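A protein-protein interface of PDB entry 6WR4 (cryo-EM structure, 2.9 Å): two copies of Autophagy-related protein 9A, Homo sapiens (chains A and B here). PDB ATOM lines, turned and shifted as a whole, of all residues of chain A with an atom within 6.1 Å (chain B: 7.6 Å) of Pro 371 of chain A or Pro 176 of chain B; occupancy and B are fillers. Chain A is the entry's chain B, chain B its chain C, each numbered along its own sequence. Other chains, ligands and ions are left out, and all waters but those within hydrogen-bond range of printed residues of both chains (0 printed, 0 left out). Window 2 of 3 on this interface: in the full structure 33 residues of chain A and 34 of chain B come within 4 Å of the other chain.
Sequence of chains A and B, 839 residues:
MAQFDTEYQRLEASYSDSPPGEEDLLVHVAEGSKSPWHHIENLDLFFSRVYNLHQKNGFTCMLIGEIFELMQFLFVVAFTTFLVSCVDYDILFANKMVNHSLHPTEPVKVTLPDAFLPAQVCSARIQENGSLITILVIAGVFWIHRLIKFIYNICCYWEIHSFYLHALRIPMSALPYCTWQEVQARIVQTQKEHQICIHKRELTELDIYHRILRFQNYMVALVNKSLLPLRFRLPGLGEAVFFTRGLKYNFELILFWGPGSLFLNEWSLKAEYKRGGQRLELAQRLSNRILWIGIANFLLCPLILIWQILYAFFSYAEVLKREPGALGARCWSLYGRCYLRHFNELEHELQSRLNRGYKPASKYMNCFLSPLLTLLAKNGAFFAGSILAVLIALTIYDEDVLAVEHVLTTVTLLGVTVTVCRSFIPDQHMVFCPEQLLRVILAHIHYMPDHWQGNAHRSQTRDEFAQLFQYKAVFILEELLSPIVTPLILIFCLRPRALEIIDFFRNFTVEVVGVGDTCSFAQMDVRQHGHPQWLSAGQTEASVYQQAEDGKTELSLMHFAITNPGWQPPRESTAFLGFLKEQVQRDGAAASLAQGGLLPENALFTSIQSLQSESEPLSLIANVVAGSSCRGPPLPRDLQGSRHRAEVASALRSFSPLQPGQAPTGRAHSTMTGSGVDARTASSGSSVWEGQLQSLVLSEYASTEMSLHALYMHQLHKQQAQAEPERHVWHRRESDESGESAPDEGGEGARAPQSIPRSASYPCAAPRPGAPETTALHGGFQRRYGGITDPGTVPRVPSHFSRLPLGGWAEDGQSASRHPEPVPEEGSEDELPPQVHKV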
ATOM      1  N   PHE A 368     -27.445   9.766  23.202  1.00  0.00           N
ATOM      2  CA  PHE A 368     -26.559  10.766  23.787  1.00  0.00           C
ATOM      3  C   PHE A 368     -25.811  11.545  22.723  1.00  0.00           C
ATOM      4  O   PHE A 368     -24.738  12.086  23.005  1.00  0.00           O
ATOM      5  CB  PHE A 368     -25.513  10.137  24.696  1.00  0.00           C
ATOM      6  CG  PHE A 368     -25.962   9.905  26.084  1.00  0.00           C
ATOM      7  CD1 PHE A 368     -25.929  10.933  27.006  1.00  0.00           C
ATOM      8  CD2 PHE A 368     -26.374   8.655  26.489  1.00  0.00           C
ATOM      9  CE1 PHE A 368     -26.324  10.719  28.302  1.00  0.00           C
ATOM     10  CE2 PHE A 368     -26.775   8.441  27.780  1.00  0.00           C
ATOM     11  CZ  PHE A 368     -26.745   9.468  28.682  1.00  0.00           C
ATOM     12  N   LEU A 369     -26.340  11.590  21.504  1.00  0.00           N
ATOM     13  CA  LEU A 369     -25.609  12.206  20.409  1.00  0.00           C
ATOM     14  C   LEU A 369     -25.551  13.720  20.585  1.00  0.00           C
ATOM     15  O   LEU A 369     -26.443  14.343  21.168  1.00  0.00           O
ATOM     16  CB  LEU A 369     -26.240  11.837  19.069  1.00  0.00           C
ATOM     17  CG  LEU A 369     -26.125  10.348  18.741  1.00  0.00           C
ATOM     18  CD1 LEU A 369     -26.873  10.005  17.464  1.00  0.00           C
ATOM     19  CD2 LEU A 369     -24.667   9.931  18.647  1.00  0.00           C
ATOM     20  N   SER A 370     -24.465  14.298  20.091  1.00  0.00           N
ATOM     21  CA  SER A 370     -24.120  15.680  20.389  1.00  0.00           C
ATOM     22  C   SER A 370     -25.079  16.621  19.677  1.00  0.00           C
ATOM     23  O   SER A 370     -25.384  16.406  18.500  1.00  0.00           O
ATOM     24  CB  SER A 370     -22.681  15.973  19.966  1.00  0.00           C
ATOM     25  OG  SER A 370     -22.318  17.315  20.236  1.00  0.00           O
ATOM     26  N   PRO A 371     -25.601  17.642  20.364  1.00  0.00           N
ATOM     27  CA  PRO A 371     -26.508  18.585  19.694  1.00  0.00           C
ATOM     28  C   PRO A 371     -25.821  19.389  18.615  1.00  0.00           C
ATOM     29  O   PRO A 371     -26.438  19.722  17.600  1.00  0.00           O
ATOM     30  CB  PRO A 371     -26.985  19.473  20.846  1.00  0.00           C
ATOM     31  CG  PRO A 371     -26.771  18.662  22.071  1.00  0.00           C
ATOM     32  CD  PRO A 371     -25.533  17.882  21.813  1.00  0.00           C
ATOM     33  N   LEU A 372     -24.546  19.695  18.805  1.00  0.00           N
ATOM     34  CA  LEU A 372     -23.757  20.387  17.806  1.00  0.00           C
ATOM     35  C   LEU A 372     -23.424  19.496  16.620  1.00  0.00           C
ATOM     36  O   LEU A 372     -23.259  20.002  15.510  1.00  0.00           O
ATOM     37  CB  LEU A 372     -22.473  20.920  18.449  1.00  0.00           C
ATOM     38  CG  LEU A 372     -21.550  21.842  17.656  1.00  0.00           C
ATOM     39  CD1 LEU A 372     -22.254  23.145  17.349  1.00  0.00           C
ATOM     40  CD2 LEU A 372     -20.267  22.098  18.421  1.00  0.00           C
ATOM     41  N   LEU A 373     -23.351  18.182  16.811  1.00  0.00           N
ATOM     42  CA  LEU A 373     -23.095  17.270  15.707  1.00  0.00           C
ATOM     43  C   LEU A 373     -24.327  16.983  14.869  1.00  0.00           C
ATOM     44  O   LEU A 373     -24.228  16.964  13.641  1.00  0.00           O
ATOM     45  CB  LEU A 373     -22.529  15.942  16.225  1.00  0.00           C
ATOM     46  CG  LEU A 373     -22.080  14.937  15.160  1.00  0.00           C
ATOM     47  CD1 LEU A 373     -20.899  15.486  14.372  1.00  0.00           C
ATOM     48  CD2 LEU A 373     -21.754  13.587  15.772  1.00  0.00           C
ATOM     49  N   THR A 374     -25.481  16.770  15.513  1.00  0.00           N
ATOM     50  CA  THR A 374     -26.743  16.570  14.806  1.00  0.00           C
ATOM     51  C   THR A 374     -27.128  17.804  13.997  1.00  0.00           C
ATOM     52  O   THR A 374     -27.646  17.693  12.881  1.00  0.00           O
ATOM     53  CB  THR A 374     -27.833  16.226  15.819  1.00  0.00           C
ATOM     54  OG1 THR A 374     -27.458  15.049  16.539  1.00  0.00           O
ATOM     55  CG2 THR A 374     -29.168  15.987  15.146  1.00  0.00           C
ATOM     56  N   LEU A 375     -26.839  18.986  14.531  1.00  0.00           N
ATOM     57  CA  LEU A 375     -27.195  20.229  13.861  1.00  0.00           C
ATOM     58  C   LEU A 375     -26.324  20.477  12.636  1.00  0.00           C
ATOM     59  O   LEU A 375     -26.784  21.050  11.645  1.00  0.00           O
ATOM     60  CB  LEU A 375     -27.061  21.367  14.858  1.00  0.00           C
ATOM     61  CG  LEU A 375     -27.447  22.799  14.574  1.00  0.00           C
ATOM     62  CD1 LEU A 375     -28.938  22.919  14.391  1.00  0.00           C
ATOM     63  CD2 LEU A 375     -26.989  23.528  15.785  1.00  0.00           C
ATOM     64  N   LEU A 376     -25.054  20.074  12.694  1.00  0.00           N
ATOM     65  CA  LEU A 376     -24.193  20.154  11.519  1.00  0.00           C
ATOM     66  C   LEU A 376     -24.500  19.041  10.526  1.00  0.00           C
ATOM     67  O   LEU A 376     -24.221  19.182   9.331  1.00  0.00           O
ATOM     68  CB  LEU A 376     -22.723  20.101  11.939  1.00  0.00           C
ATOM     69  CG  LEU A 376     -21.916  21.376  12.212  1.00  0.00           C
ATOM     70  CD1 LEU A 376     -21.734  22.153  10.919  1.00  0.00           C
ATOM     71  CD2 LEU A 376     -22.534  22.266  13.279  1.00  0.00           C
ATOM     72  N   LEU B  53     -34.135  28.235  25.307  1.00  0.00           N
ATOM     73  CA  LEU B  53     -32.684  28.108  25.385  1.00  0.00           C
ATOM     74  C   LEU B  53     -32.311  26.702  25.831  1.00  0.00           C
ATOM     75  O   LEU B  53     -31.293  26.150  25.403  1.00  0.00           O
ATOM     76  CB  LEU B  53     -32.129  29.176  26.331  1.00  0.00           C
ATOM     77  CG  LEU B  53     -30.690  29.706  26.286  1.00  0.00           C
ATOM     78  CD1 LEU B  53     -29.696  28.810  26.965  1.00  0.00           C
ATOM     79  CD2 LEU B  53     -30.279  29.965  24.852  1.00  0.00           C
ATOM     80  N   HIS B  54     -33.156  26.090  26.662  1.00  0.00           N
ATOM     81  CA  HIS B  54     -32.944  24.720  27.105  1.00  0.00           C
ATOM     82  C   HIS B  54     -33.218  23.701  26.013  1.00  0.00           C
ATOM     83  O   HIS B  54     -32.527  22.681  25.950  1.00  0.00           O
ATOM     84  CB  HIS B  54     -33.828  24.427  28.309  1.00  0.00           C
ATOM     85  CG  HIS B  54     -33.744  23.015  28.793  1.00  0.00           C
ATOM     86  ND1 HIS B  54     -32.633  22.511  29.430  1.00  0.00           N
ATOM     87  CD2 HIS B  54     -34.644  22.006  28.755  1.00  0.00           C
ATOM     88  CE1 HIS B  54     -32.847  21.248  29.750  1.00  0.00           C
ATOM     89  NE2 HIS B  54     -34.061  20.917  29.353  1.00  0.00           N
ATOM     90  N   GLN B  55     -34.209  23.945  25.161  1.00  0.00           N
ATOM     91  CA  GLN B  55     -34.581  22.998  24.122  1.00  0.00           C
ATOM     92  C   GLN B  55     -33.710  23.102  22.888  1.00  0.00           C
ATOM     93  O   GLN B  55     -33.619  22.137  22.128  1.00  0.00           O
ATOM     94  CB  GLN B  55     -36.043  23.190  23.731  1.00  0.00           C
ATOM     95  CG  GLN B  55     -36.985  22.902  24.859  1.00  0.00           C
ATOM     96  CD  GLN B  55     -36.918  21.468  25.312  1.00  0.00           C
ATOM     97  OE1 GLN B  55     -36.831  20.554  24.501  1.00  0.00           O
ATOM     98  NE2 GLN B  55     -36.943  21.263  26.615  1.00  0.00           N
ATOM     99  N   LYS B  56     -33.082  24.246  22.668  1.00  0.00           N
ATOM    100  CA  LYS B  56     -32.063  24.381  21.650  1.00  0.00           C
ATOM    101  C   LYS B  56     -30.677  24.017  22.147  1.00  0.00           C
ATOM    102  O   LYS B  56     -29.702  24.274  21.433  1.00  0.00           O
ATOM    103  CB  LYS B  56     -32.045  25.812  21.102  1.00  0.00           C
ATOM    104  CG  LYS B  56     -33.282  26.206  20.334  1.00  0.00           C
ATOM    105  CD  LYS B  56     -33.348  25.475  19.012  1.00  0.00           C
ATOM    106  CE  LYS B  56     -34.529  25.938  18.190  1.00  0.00           C
ATOM    107  NZ  LYS B  56     -34.316  27.335  17.732  1.00  0.00           N
ATOM    108  N   ASN B  57     -30.569  23.481  23.369  1.00  0.00           N
ATOM    109  CA  ASN B  57     -29.386  22.846  23.946  1.00  0.00           C
ATOM    110  C   ASN B  57     -28.242  23.820  24.191  1.00  0.00           C
ATOM    111  O   ASN B  57     -27.080  23.409  24.231  1.00  0.00           O
ATOM    112  CB  ASN B  57     -28.910  21.681  23.077  1.00  0.00           C
ATOM    113  CG  ASN B  57     -29.880  20.529  23.077  1.00  0.00           C
ATOM    114  OD1 ASN B  57     -30.429  20.166  24.111  1.00  0.00           O
ATOM    115  ND2 ASN B  57     -30.106  19.950  21.909  1.00  0.00           N
ATOM    116  N   GLY B  58     -28.537  25.109  24.311  1.00  0.00           N
ATOM    117  CA  GLY B  58     -27.558  26.075  24.757  1.00  0.00           C
ATOM    118  C   GLY B  58     -27.583  27.344  23.938  1.00  0.00           C
ATOM    119  O   GLY B  58     -28.335  27.487  22.976  1.00  0.00           O
ATOM    120  N   CYS B  61     -25.263  26.600  20.642  1.00  0.00           N
ATOM    121  CA  CYS B  61     -25.899  25.640  19.749  1.00  0.00           C
ATOM    122  C   CYS B  61     -27.075  26.282  19.026  1.00  0.00           C
ATOM    123  O   CYS B  61     -27.286  26.056  17.830  1.00  0.00           O
ATOM    124  CB  CYS B  61     -26.336  24.408  20.538  1.00  0.00           C
ATOM    125  SG  CYS B  61     -26.936  23.061  19.518  1.00  0.00           S
ATOM    126  N   ILE B  64     -25.415  28.963  16.396  1.00  0.00           N
ATOM    127  CA  ILE B  64     -24.978  28.372  15.137  1.00  0.00           C
ATOM    128  C   ILE B  64     -26.123  27.615  14.475  1.00  0.00           C
ATOM    129  O   ILE B  64     -26.066  27.340  13.273  1.00  0.00           O
ATOM    130  CB  ILE B  64     -23.740  27.479  15.371  1.00  0.00           C
ATOM    131  CG1 ILE B  64     -22.930  27.304  14.085  1.00  0.00           C
ATOM    132  CG2 ILE B  64     -24.123  26.128  15.929  1.00  0.00           C
ATOM    133  CD1 ILE B  64     -22.206  28.558  13.659  1.00  0.00           C
ATOM    134  N   ILE B 170     -25.744  26.947  36.121  1.00  0.00           N
ATOM    135  CA  ILE B 170     -25.740  25.847  35.163  1.00  0.00           C
ATOM    136  C   ILE B 170     -24.937  26.290  33.944  1.00  0.00           C
ATOM    137  O   ILE B 170     -25.335  27.230  33.263  1.00  0.00           O
ATOM    138  CB  ILE B 170     -27.158  25.413  34.745  1.00  0.00           C
ATOM    139  CG1 ILE B 170     -27.917  24.840  35.943  1.00  0.00           C
ATOM    140  CG2 ILE B 170     -27.083  24.378  33.644  1.00  0.00           C
ATOM    141  CD1 ILE B 170     -29.377  24.568  35.674  1.00  0.00           C
ATOM    142  N   PRO B 171     -23.806  25.652  33.653  1.00  0.00           N
ATOM    143  CA  PRO B 171     -23.021  26.032  32.474  1.00  0.00           C
ATOM    144  C   PRO B 171     -23.675  25.567  31.181  1.00  0.00           C
ATOM    145  O   PRO B 171     -24.654  24.822  31.175  1.00  0.00           O
ATOM    146  CB  PRO B 171     -21.687  25.312  32.695  1.00  0.00           C
ATOM    147  CG  PRO B 171     -21.643  25.026  34.159  1.00  0.00           C
ATOM    148  CD  PRO B 171     -23.057  24.753  34.543  1.00  0.00           C
ATOM    149  N   MET B 172     -23.099  26.023  30.066  1.00  0.00           N
ATOM    150  CA  MET B 172     -23.559  25.580  28.755  1.00  0.00           C
ATOM    151  C   MET B 172     -23.096  24.175  28.419  1.00  0.00           C
ATOM    152  O   MET B 172     -23.592  23.597  27.445  1.00  0.00           O
ATOM    153  CB  MET B 172     -23.079  26.529  27.661  1.00  0.00           C
ATOM    154  CG  MET B 172     -23.678  27.914  27.687  1.00  0.00           C
ATOM    155  SD  MET B 172     -25.454  28.008  27.403  1.00  0.00           S
ATOM    156  CE  MET B 172     -26.050  28.413  29.040  1.00  0.00           C
ATOM    157  N   SER B 173     -22.142  23.627  29.172  1.00  0.00           N
ATOM    158  CA  SER B 173     -21.758  22.236  28.981  1.00  0.00           C
ATOM    159  C   SER B 173     -22.738  21.306  29.678  1.00  0.00           C
ATOM    160  O   SER B 173     -23.087  20.249  29.143  1.00  0.00           O
ATOM    161  CB  SER B 173     -20.341  22.006  29.499  1.00  0.00           C
ATOM    162  OG  SER B 173     -20.283  22.186  30.903  1.00  0.00           O
ATOM    163  N   ALA B 174     -23.207  21.693  30.863  1.00  0.00           N
ATOM    164  CA  ALA B 174     -24.118  20.839  31.613  1.00  0.00           C
ATOM    165  C   ALA B 174     -25.552  21.000  31.134  1.00  0.00           C
ATOM    166  O   ALA B 174     -26.428  20.218  31.512  1.00  0.00           O
ATOM    167  CB  ALA B 174     -24.018  21.150  33.102  1.00  0.00           C
ATOM    168  N   LEU B 175     -25.809  22.004  30.300  1.00  0.00           N
ATOM    169  CA  LEU B 175     -27.183  22.303  29.902  1.00  0.00           C
ATOM    170  C   LEU B 175     -27.818  21.288  28.945  1.00  0.00           C
ATOM    171  O   LEU B 175     -28.994  20.953  29.171  1.00  0.00           O
ATOM    172  CB  LEU B 175     -27.256  23.730  29.339  1.00  0.00           C
ATOM    173  CG  LEU B 175     -28.646  24.241  28.983  1.00  0.00           C
ATOM    174  CD1 LEU B 175     -29.509  24.277  30.218  1.00  0.00           C
ATOM    175  CD2 LEU B 175     -28.544  25.604  28.380  1.00  0.00           C
ATOM    176  N   PRO B 176     -27.149  20.747  27.902  1.00  0.00           N
ATOM    177  CA  PRO B 176     -27.812  19.678  27.125  1.00  0.00           C
ATOM    178  C   PRO B 176     -28.008  18.379  27.887  1.00  0.00           C
ATOM    179  O   PRO B 176     -28.739  17.500  27.416  1.00  0.00           O
ATOM    180  CB  PRO B 176     -26.870  19.470  25.933  1.00  0.00           C
ATOM    181  CG  PRO B 176     -26.131  20.694  25.817  1.00  0.00           C
ATOM    182  CD  PRO B 176     -25.923  21.181  27.199  1.00  0.00           C
ATOM    183  N   TYR B 177     -27.377  18.226  29.045  1.00  0.00           N
ATOM    184  CA  TYR B 177     -27.452  17.009  29.829  1.00  0.00           C
ATOM    185  C   TYR B 177     -28.289  17.193  31.084  1.00  0.00           C
ATOM    186  O   TYR B 177     -28.262  16.336  31.974  1.00  0.00           O
ATOM    187  CB  TYR B 177     -26.037  16.537  30.160  1.00  0.00           C
ATOM    188  CG  TYR B 177     -25.234  16.319  28.900  1.00  0.00           C
ATOM    189  CD1 TYR B 177     -25.403  15.173  28.140  1.00  0.00           C
ATOM    190  CD2 TYR B 177     -24.333  17.276  28.452  1.00  0.00           C
ATOM    191  CE1 TYR B 177     -24.689  14.978  26.978  1.00  0.00           C
ATOM    192  CE2 TYR B 177     -23.617  17.092  27.286  1.00  0.00           C
ATOM    193  CZ  TYR B 177     -23.798  15.938  26.557  1.00  0.00           C
ATOM    194  OH  TYR B 177     -23.090  15.738  25.400  1.00  0.00           O
ATOM    195  N   CYS B 178     -29.024  18.297  31.169  1.00  0.00           N
ATOM    196  CA  CYS B 178     -30.069  18.494  32.159  1.00  0.00           C
ATOM    197  C   CYS B 178     -31.423  18.223  31.524  1.00  0.00           C
ATOM    198  O   CYS B 178     -31.590  18.326  30.307  1.00  0.00           O
ATOM    199  CB  CYS B 178     -30.060  19.920  32.723  1.00  0.00           C
ATOM    200  SG  CYS B 178     -28.699  20.342  33.817  1.00  0.00           S
ATOM    201  N   THR B 179     -32.384  17.868  32.361  1.00  0.00           N
ATOM    202  CA  THR B 179     -33.771  17.803  31.947  1.00  0.00           C
ATOM    203  C   THR B 179     -34.434  19.141  32.239  1.00  0.00           C
ATOM    204  O   THR B 179     -33.817  20.033  32.820  1.00  0.00           O
ATOM    205  CB  THR B 179     -34.490  16.675  32.675  1.00  0.00           C
ATOM    206  OG1 THR B 179     -34.484  16.940  34.079  1.00  0.00           O
ATOM    207  CG2 THR B 179     -33.770  15.374  32.425  1.00  0.00           C
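Of the 9 printed residues of chain A, 3 touch a printed residue of chain B.
Hydrophobic or aromatic side chains of chain A that line the printed part of chain B: Pro 371, Leu 372 and Leu 375.
Of the 18 printed residues of chain B, 4 touch a printed residue of chain A.
Printed residues of chain B that touch a printed residue of chain A: Asn 57, Cys 61, Ile 64 and Pro 176.
Hydrophobic or aromatic side chains of chain B that line the printed part of chain A: Ile 64 and Pro 176.
Among the printed residues, 6 pairs touch across the chains.
Among the printed residues, no Asp or Glu carboxylate lies within 4 Å of a Lys or Arg side-chain nitrogen of the other chain.
No residue of chain B comes within 4 Å of Ser 370 of chain A.
Printed residues of chain B within 4 Å of Pro 371 of chain A: Asn 57, Cys 61 and Pro 176.
Printed residues of chain B within 4 Å of Leu 372 of chain A: Ile 64.
Leu 376 of chain A touches none of the printed residues of chain B.
Leu 53 of chain B touches none of the printed residues of chain A.
Of the printed residues of chain A, Cys 61 of chain B touches Pro 371 and Leu 375.
Of the printed residues of chain A, Ile 64 of chain B touches Leu 372 (3.8 Å) and Leu 375 (3.9 Å).
Of chain A, only Pro 371 (3.9 Å) comes within 4 Å of Pro 176 of chain B.
No position is printed for both chains.
Of the 6 pairs that touch across the chains among the printed residues, none has its exchanged pair printed and touching as well.
The backbone carbonyl oxygen (O) of Lys 56 of chain B lies close to the side-chain sulfur (SG) of Cys 61 of chain B, 3.6 Å away.
Among the printed residues, merely in contact across the chains: Leu 375 of chain A with Cys 61 of chain B (3.3 Å), Pro 371 of chain A with Asn 57 of chain B (3.3 Å), Leu 372 of chain A with Ile 64 of chain B (3.8 Å), Pro 371 of chain A with Cys 61 of chain B (3.8 Å), Leu 375 of chain A with Ile 64 of chain B (3.9 Å) and Pro 371 of chain A with Pro 176 of chain B (3.9 Å).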
